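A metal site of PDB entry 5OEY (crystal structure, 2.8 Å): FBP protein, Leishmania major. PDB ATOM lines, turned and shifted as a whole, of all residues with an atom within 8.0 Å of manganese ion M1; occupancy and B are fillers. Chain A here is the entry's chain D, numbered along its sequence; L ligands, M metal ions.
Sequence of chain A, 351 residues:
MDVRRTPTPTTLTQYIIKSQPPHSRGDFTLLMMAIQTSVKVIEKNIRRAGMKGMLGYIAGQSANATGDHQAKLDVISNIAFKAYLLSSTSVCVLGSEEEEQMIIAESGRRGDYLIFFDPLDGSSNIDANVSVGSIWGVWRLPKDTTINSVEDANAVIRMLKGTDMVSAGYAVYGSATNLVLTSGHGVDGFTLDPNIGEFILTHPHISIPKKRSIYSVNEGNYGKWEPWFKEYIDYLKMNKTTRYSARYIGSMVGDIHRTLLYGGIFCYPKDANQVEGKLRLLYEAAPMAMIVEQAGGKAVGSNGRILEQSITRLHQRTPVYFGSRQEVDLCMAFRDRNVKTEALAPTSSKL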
ATOM      1  N   ASP A  74     -30.022   5.153   4.554  1.00  0.00           N
ATOM      2  CA  ASP A  74     -30.145   3.701   4.607  1.00  0.00           C
ATOM      3  C   ASP A  74     -31.610   3.286   4.465  1.00  0.00           C
ATOM      4  O   ASP A  74     -31.951   2.339   3.751  1.00  0.00           O
ATOM      5  CB  ASP A  74     -29.633   3.126   5.933  1.00  0.00           C
ATOM      6  CG  ASP A  74     -28.148   3.084   6.003  1.00  0.00           C
ATOM      7  OD1 ASP A  74     -27.595   4.165   6.222  1.00  0.00           O
ATOM      8  OD2 ASP A  74     -27.537   2.011   5.894  1.00  0.00           O
ATOM      9  N   GLU A  97     -29.555  -6.038   3.831  1.00  0.00           N
ATOM     10  CA  GLU A  97     -28.747  -5.753   5.017  1.00  0.00           C
ATOM     11  C   GLU A  97     -29.504  -5.019   6.124  1.00  0.00           C
ATOM     12  O   GLU A  97     -29.230  -5.223   7.295  1.00  0.00           O
ATOM     13  CB  GLU A  97     -27.616  -4.862   4.596  1.00  0.00           C
ATOM     14  CG  GLU A  97     -26.538  -4.600   5.619  1.00  0.00           C
ATOM     15  CD  GLU A  97     -25.385  -3.942   4.934  1.00  0.00           C
ATOM     16  OE1 GLU A  97     -24.559  -4.636   4.379  1.00  0.00           O
ATOM     17  OE2 GLU A  97     -25.370  -2.727   4.868  1.00  0.00           O
ATOM     18  N   GLU A  98     -30.445  -4.152   5.752  1.00  0.00           N
ATOM     19  CA  GLU A  98     -31.216  -3.350   6.727  1.00  0.00           C
ATOM     20  C   GLU A  98     -32.326  -4.139   7.455  1.00  0.00           C
ATOM     21  O   GLU A  98     -33.012  -3.573   8.305  1.00  0.00           O
ATOM     22  CB  GLU A  98     -31.837  -2.106   6.038  1.00  0.00           C
ATOM     23  CG  GLU A  98     -30.877  -1.229   5.223  1.00  0.00           C
ATOM     24  CD  GLU A  98     -29.578  -0.917   5.962  1.00  0.00           C
ATOM     25  OE1 GLU A  98     -29.650  -0.590   7.171  1.00  0.00           O
ATOM     26  OE2 GLU A  98     -28.492  -0.981   5.344  1.00  0.00           O
ATOM     27  N   PHE A 117     -29.301  -7.721  -1.142  1.00  0.00           N
ATOM     28  CA  PHE A 117     -28.700  -6.426  -1.447  1.00  0.00           C
ATOM     29  C   PHE A 117     -28.305  -5.596  -0.238  1.00  0.00           C
ATOM     30  O   PHE A 117     -28.908  -5.690   0.837  1.00  0.00           O
ATOM     31  CB  PHE A 117     -29.621  -5.645  -2.369  1.00  0.00           C
ATOM     32  CG  PHE A 117     -30.972  -5.369  -1.791  1.00  0.00           C
ATOM     33  CD1 PHE A 117     -32.024  -6.247  -1.980  1.00  0.00           C
ATOM     34  CD2 PHE A 117     -31.203  -4.202  -1.055  1.00  0.00           C
ATOM     35  CE1 PHE A 117     -33.281  -5.983  -1.431  1.00  0.00           C
ATOM     36  CE2 PHE A 117     -32.444  -3.934  -0.521  1.00  0.00           C
ATOM     37  CZ  PHE A 117     -33.493  -4.836  -0.714  1.00  0.00           C
ATOM     38  N   ASP A 118     -27.249  -4.805  -0.419  1.00  0.00           N
ATOM     39  CA  ASP A 118     -26.898  -3.750   0.503  1.00  0.00           C
ATOM     40  C   ASP A 118     -27.405  -2.485  -0.197  1.00  0.00           C
ATOM     41  O   ASP A 118     -26.729  -1.984  -1.090  1.00  0.00           O
ATOM     42  CB  ASP A 118     -25.381  -3.715   0.753  1.00  0.00           C
ATOM     43  CG  ASP A 118     -24.952  -2.652   1.742  1.00  0.00           C
ATOM     44  OD1 ASP A 118     -25.823  -1.925   2.319  1.00  0.00           O
ATOM     45  OD2 ASP A 118     -23.742  -2.484   1.944  1.00  0.00           O
ATOM     46  N   PRO A 119     -28.572  -1.946   0.199  1.00  0.00           N
ATOM     47  CA  PRO A 119     -29.109  -0.801  -0.502  1.00  0.00           C
ATOM     48  C   PRO A 119     -28.262   0.471  -0.438  1.00  0.00           C
ATOM     49  O   PRO A 119     -28.371   1.330  -1.327  1.00  0.00           O
ATOM     50  CB  PRO A 119     -30.458  -0.594   0.173  1.00  0.00           C
ATOM     51  CG  PRO A 119     -30.201  -0.985   1.576  1.00  0.00           C
ATOM     52  CD  PRO A 119     -29.295  -2.167   1.463  1.00  0.00           C
ATOM     53  N   LEU A 120     -27.467   0.640   0.618  1.00  0.00           N
ATOM     54  CA  LEU A 120     -26.559   1.775   0.716  1.00  0.00           C
ATOM     55  C   LEU A 120     -25.342   1.395   1.527  1.00  0.00           C
ATOM     56  O   LEU A 120     -25.398   1.270   2.736  1.00  0.00           O
ATOM     57  CB  LEU A 120     -27.222   3.026   1.311  1.00  0.00           C
ATOM     58  CG  LEU A 120     -26.404   4.314   1.271  1.00  0.00           C
ATOM     59  CD1 LEU A 120     -26.057   4.718  -0.159  1.00  0.00           C
ATOM     60  CD2 LEU A 120     -27.201   5.442   1.878  1.00  0.00           C
ATOM     61  N   ASP A 121     -24.223   1.243   0.830  1.00  0.00           N
ATOM     62  CA  ASP A 121     -22.969   0.877   1.447  1.00  0.00           C
ATOM     63  C   ASP A 121     -22.166   2.150   1.721  1.00  0.00           C
ATOM     64  O   ASP A 121     -21.946   2.986   0.803  1.00  0.00           O
ATOM     65  CB  ASP A 121     -22.178  -0.081   0.557  1.00  0.00           C
ATOM     66  CG  ASP A 121     -20.973  -0.714   1.354  1.00  0.00           C
ATOM     67  OD1 ASP A 121     -21.248  -1.365   2.409  1.00  0.00           O
ATOM     68  OD2 ASP A 121     -19.758  -0.550   0.947  1.00  0.00           O
ATOM     69  N   GLY A 122     -21.653   2.257   2.943  1.00  0.00           N
ATOM     70  CA  GLY A 122     -20.766   3.364   3.289  1.00  0.00           C
ATOM     71  C   GLY A 122     -21.617   4.539   3.727  1.00  0.00           C
ATOM     72  O   GLY A 122     -21.253   5.652   3.425  1.00  0.00           O
ATOM     73  N   SER A 123     -22.731   4.315   4.406  1.00  0.00           N
ATOM     74  CA  SER A 123     -23.635   5.443   4.805  1.00  0.00           C
ATOM     75  C   SER A 123     -23.095   6.459   5.788  1.00  0.00           C
ATOM     76  O   SER A 123     -23.590   7.521   5.846  1.00  0.00           O
ATOM     77  CB  SER A 123     -24.966   4.921   5.305  1.00  0.00           C
ATOM     78  OG  SER A 123     -25.093   3.574   5.044  1.00  0.00           O
ATOM     79  N   GLY A 133     -22.231   3.435  -2.250  1.00  0.00           N
ATOM     80  CA  GLY A 133     -22.716   2.554  -3.282  1.00  0.00           C
ATOM     81  C   GLY A 133     -23.855   1.643  -2.848  1.00  0.00           C
ATOM     82  O   GLY A 133     -24.419   1.814  -1.782  1.00  0.00           O
ATOM     83  N   ILE A 135     -25.091  -2.624  -3.475  1.00  0.00           N
ATOM     84  CA  ILE A 135     -24.539  -3.914  -3.911  1.00  0.00           C
ATOM     85  C   ILE A 135     -25.686  -4.915  -3.969  1.00  0.00           C
ATOM     86  O   ILE A 135     -26.529  -4.894  -3.093  1.00  0.00           O
ATOM     87  CB  ILE A 135     -23.447  -4.447  -2.957  1.00  0.00           C
ATOM     88  CG1 ILE A 135     -22.341  -3.405  -2.762  1.00  0.00           C
ATOM     89  CG2 ILE A 135     -22.801  -5.692  -3.528  1.00  0.00           C
ATOM     90  CD1 ILE A 135     -21.433  -3.674  -1.574  1.00  0.00           C
ATOM     91  N   MET A 252     -16.374   0.536   0.639  1.00  0.00           N
ATOM     92  CA  MET A 252     -16.036  -0.680  -0.067  1.00  0.00           C
ATOM     93  C   MET A 252     -16.308  -0.587  -1.576  1.00  0.00           C
ATOM     94  O   MET A 252     -15.504  -1.063  -2.364  1.00  0.00           O
ATOM     95  CB  MET A 252     -16.824  -1.848   0.509  1.00  0.00           C
ATOM     96  CG  MET A 252     -16.383  -3.197   0.007  1.00  0.00           C
ATOM     97  SD  MET A 252     -17.751  -4.378   0.066  1.00  0.00           S
ATOM     98  CE  MET A 252     -18.435  -3.907   1.661  1.00  0.00           C
ATOM     99  N   VAL A 253     -17.460  -0.050  -1.961  1.00  0.00           N
ATOM    100  CA  VAL A 253     -17.802   0.034  -3.366  1.00  0.00           C
ATOM    101  C   VAL A 253     -16.814   0.996  -4.055  1.00  0.00           C
ATOM    102  O   VAL A 253     -16.245   0.671  -5.087  1.00  0.00           O
ATOM    103  CB  VAL A 253     -19.259   0.465  -3.590  1.00  0.00           C
ATOM    104  CG1 VAL A 253     -19.508   0.779  -5.055  1.00  0.00           C
ATOM    105  CG2 VAL A 253     -20.247  -0.609  -3.124  1.00  0.00           C
ATOM    106  N   LYS A 278     -15.207  -8.111   9.052  1.00  0.00           N
ATOM    107  CA  LYS A 278     -16.144  -6.964   9.012  1.00  0.00           C
ATOM    108  C   LYS A 278     -17.242  -7.096   7.937  1.00  0.00           C
ATOM    109  O   LYS A 278     -18.413  -6.824   8.202  1.00  0.00           O
ATOM    110  CB  LYS A 278     -15.386  -5.636   8.789  1.00  0.00           C
ATOM    111  CG  LYS A 278     -16.253  -4.372   9.011  1.00  0.00           C
ATOM    112  CD  LYS A 278     -17.113  -3.804   7.863  1.00  0.00           C
ATOM    113  CE  LYS A 278     -17.371  -2.256   7.946  1.00  0.00           C
ATOM    114  NZ  LYS A 278     -18.348  -1.678   6.963  1.00  0.00           N
ATOM    115  N   LEU A 279     -16.852  -7.525   6.751  1.00  0.00           N
ATOM    116  CA  LEU A 279     -17.766  -7.577   5.611  1.00  0.00           C
ATOM    117  C   LEU A 279     -18.689  -8.766   5.671  1.00  0.00           C
ATOM    118  O   LEU A 279     -18.307  -9.842   6.083  1.00  0.00           O
ATOM    119  CB  LEU A 279     -17.002  -7.622   4.300  1.00  0.00           C
ATOM    120  CG  LEU A 279     -16.534  -6.276   3.753  1.00  0.00           C
ATOM    121  CD1 LEU A 279     -15.628  -5.541   4.718  1.00  0.00           C
ATOM    122  CD2 LEU A 279     -15.821  -6.461   2.418  1.00  0.00           C
ATOM    123  N   ARG A 280     -19.902  -8.573   5.199  1.00  0.00           N
ATOM    124  CA  ARG A 280     -20.909  -9.596   5.187  1.00  0.00           C
ATOM    125  C   ARG A 280     -20.811 -10.421   3.935  1.00  0.00           C
ATOM    126  O   ARG A 280     -20.606  -9.900   2.851  1.00  0.00           O
ATOM    127  CB  ARG A 280     -22.291  -8.944   5.276  1.00  0.00           C
ATOM    128  CG  ARG A 280     -22.579  -8.398   6.671  1.00  0.00           C
ATOM    129  CD  ARG A 280     -24.024  -8.052   6.750  1.00  0.00           C
ATOM    130  NE  ARG A 280     -24.423  -7.492   8.033  1.00  0.00           N
ATOM    131  CZ  ARG A 280     -24.186  -6.227   8.411  1.00  0.00           C
ATOM    132  NH1 ARG A 280     -23.513  -5.384   7.624  1.00  0.00           N
ATOM    133  NH2 ARG A 280     -24.610  -5.778   9.580  1.00  0.00           N
ATOM    134  N   TYR A 283     -24.471 -10.157   1.015  1.00  0.00           N
ATOM    135  CA  TYR A 283     -24.835  -8.912   0.325  1.00  0.00           C
ATOM    136  C   TYR A 283     -23.650  -7.909   0.181  1.00  0.00           C
ATOM    137  O   TYR A 283     -23.845  -6.775  -0.313  1.00  0.00           O
ATOM    138  CB  TYR A 283     -26.139  -8.234   0.849  1.00  0.00           C
ATOM    139  CG  TYR A 283     -26.875  -8.788   2.096  1.00  0.00           C
ATOM    140  CD1 TYR A 283     -26.284  -8.861   3.338  1.00  0.00           C
ATOM    141  CD2 TYR A 283     -28.203  -9.301   1.982  1.00  0.00           C
ATOM    142  CE1 TYR A 283     -26.967  -9.379   4.422  1.00  0.00           C
ATOM    143  CE2 TYR A 283     -28.893  -9.859   3.046  1.00  0.00           C
ATOM    144  CZ  TYR A 283     -28.280  -9.884   4.265  1.00  0.00           C
ATOM    145  OH  TYR A 283     -28.982 -10.446   5.323  1.00  0.00           O
ATOM    146  N   GLU A 284     -22.424  -8.339   0.476  1.00  0.00           N
ATOM    147  CA  GLU A 284     -21.223  -7.526   0.218  1.00  0.00           C
ATOM    148  C   GLU A 284     -20.110  -8.345  -0.472  1.00  0.00           C
ATOM    149  O   GLU A 284     -19.772  -8.092  -1.623  1.00  0.00           O
ATOM    150  CB  GLU A 284     -20.706  -6.883   1.508  1.00  0.00           C
ATOM    151  CG  GLU A 284     -21.693  -5.892   2.114  1.00  0.00           C
ATOM    152  CD  GLU A 284     -21.250  -5.296   3.452  1.00  0.00           C
ATOM    153  OE1 GLU A 284     -20.530  -5.965   4.230  1.00  0.00           O
ATOM    154  OE2 GLU A 284     -21.602  -4.104   3.719  1.00  0.00           O
ATOM    155  N   ARG A 317     -20.357 -13.208   8.330  1.00  0.00           N
ATOM    156  CA  ARG A 317     -19.206 -12.375   7.927  1.00  0.00           C
ATOM    157  C   ARG A 317     -17.970 -13.126   7.475  1.00  0.00           C
ATOM    158  O   ARG A 317     -17.851 -14.348   7.683  1.00  0.00           O
ATOM    159  CB  ARG A 317     -18.765 -11.480   9.049  1.00  0.00           C
ATOM    160  CG  ARG A 317     -19.884 -10.633   9.522  1.00  0.00           C
ATOM    161  CD  ARG A 317     -19.391  -9.586  10.448  1.00  0.00           C
ATOM    162  NE  ARG A 317     -20.702  -9.199  10.960  1.00  0.00           N
ATOM    163  CZ  ARG A 317     -21.414  -8.115  10.619  1.00  0.00           C
ATOM    164  NH1 ARG A 317     -20.900  -7.106   9.922  1.00  0.00           N
ATOM    165  NH2 ARG A 317     -22.645  -8.017  11.107  1.00  0.00           N
HETATM  166  P1  LIG L   1     -23.509  -0.040   5.707  1.00  0.00           P
HETATM  167  O1  LIG L   1     -22.179   0.522   6.193  1.00  0.00           O
HETATM  168  O2  LIG L   1     -24.372   1.105   5.326  1.00  0.00           O
HETATM  169  O3  LIG L   1     -24.256  -0.773   6.779  1.00  0.00           O
HETATM  170  O4  LIG L   1     -23.311  -0.862   4.464  1.00  0.00           O
HETATM  171 MN    MN M   1     -22.793  -2.646   3.938  1.00  0.00          MN
HETATM  172 MN    MN M   2     -26.860  -0.061   7.450  1.00  0.00          MN
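Manganese ion M1 is bound by the side-chain carboxylate (OE2) of Glu 284 (1.9 Å), an oxygen (O4) of the ligand (1.9 Å), the side-chain carboxylate (OD2) of Asp 118 (2.2 Å), the side-chain carboxylate (OD1) of Asp 121 (2.5 Å) and the side-chain carboxylate (OE1) of Glu 97 (2.7 Å).
Slightly farther from manganese ion M1 lies the side-chain carboxylate (OE2) of Glu 97 (2.7 Å).
The guanidinium group of Arg 280 sits close to the side-chain carboxylate of Glu 97 (3.5 Å).
OD1 of Asp 118 lies close to N of Leu 120.
The backbone NH (N) of Glu 97 sits at hydrogen-bond distance from the backbone carbonyl oxygen (O) of Phe 117 (3.1 Å).
The backbone NH of Asp 121 lies within hydrogen-bond range of the backbone carbonyl oxygen of Gly 133, 2.7 Å away.
The side-chain carboxylate of Glu 284 is in hydrogen-bond range of the backbone NH of Arg 280 (2.9 Å).
The backbone NH (N) of Asp 118 sits at hydrogen-bond distance from the backbone carbonyl oxygen (O) of Ile 135 (2.8 Å).
Of the 20 residues printed, 4 come within 4 Å of manganese ion M1.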
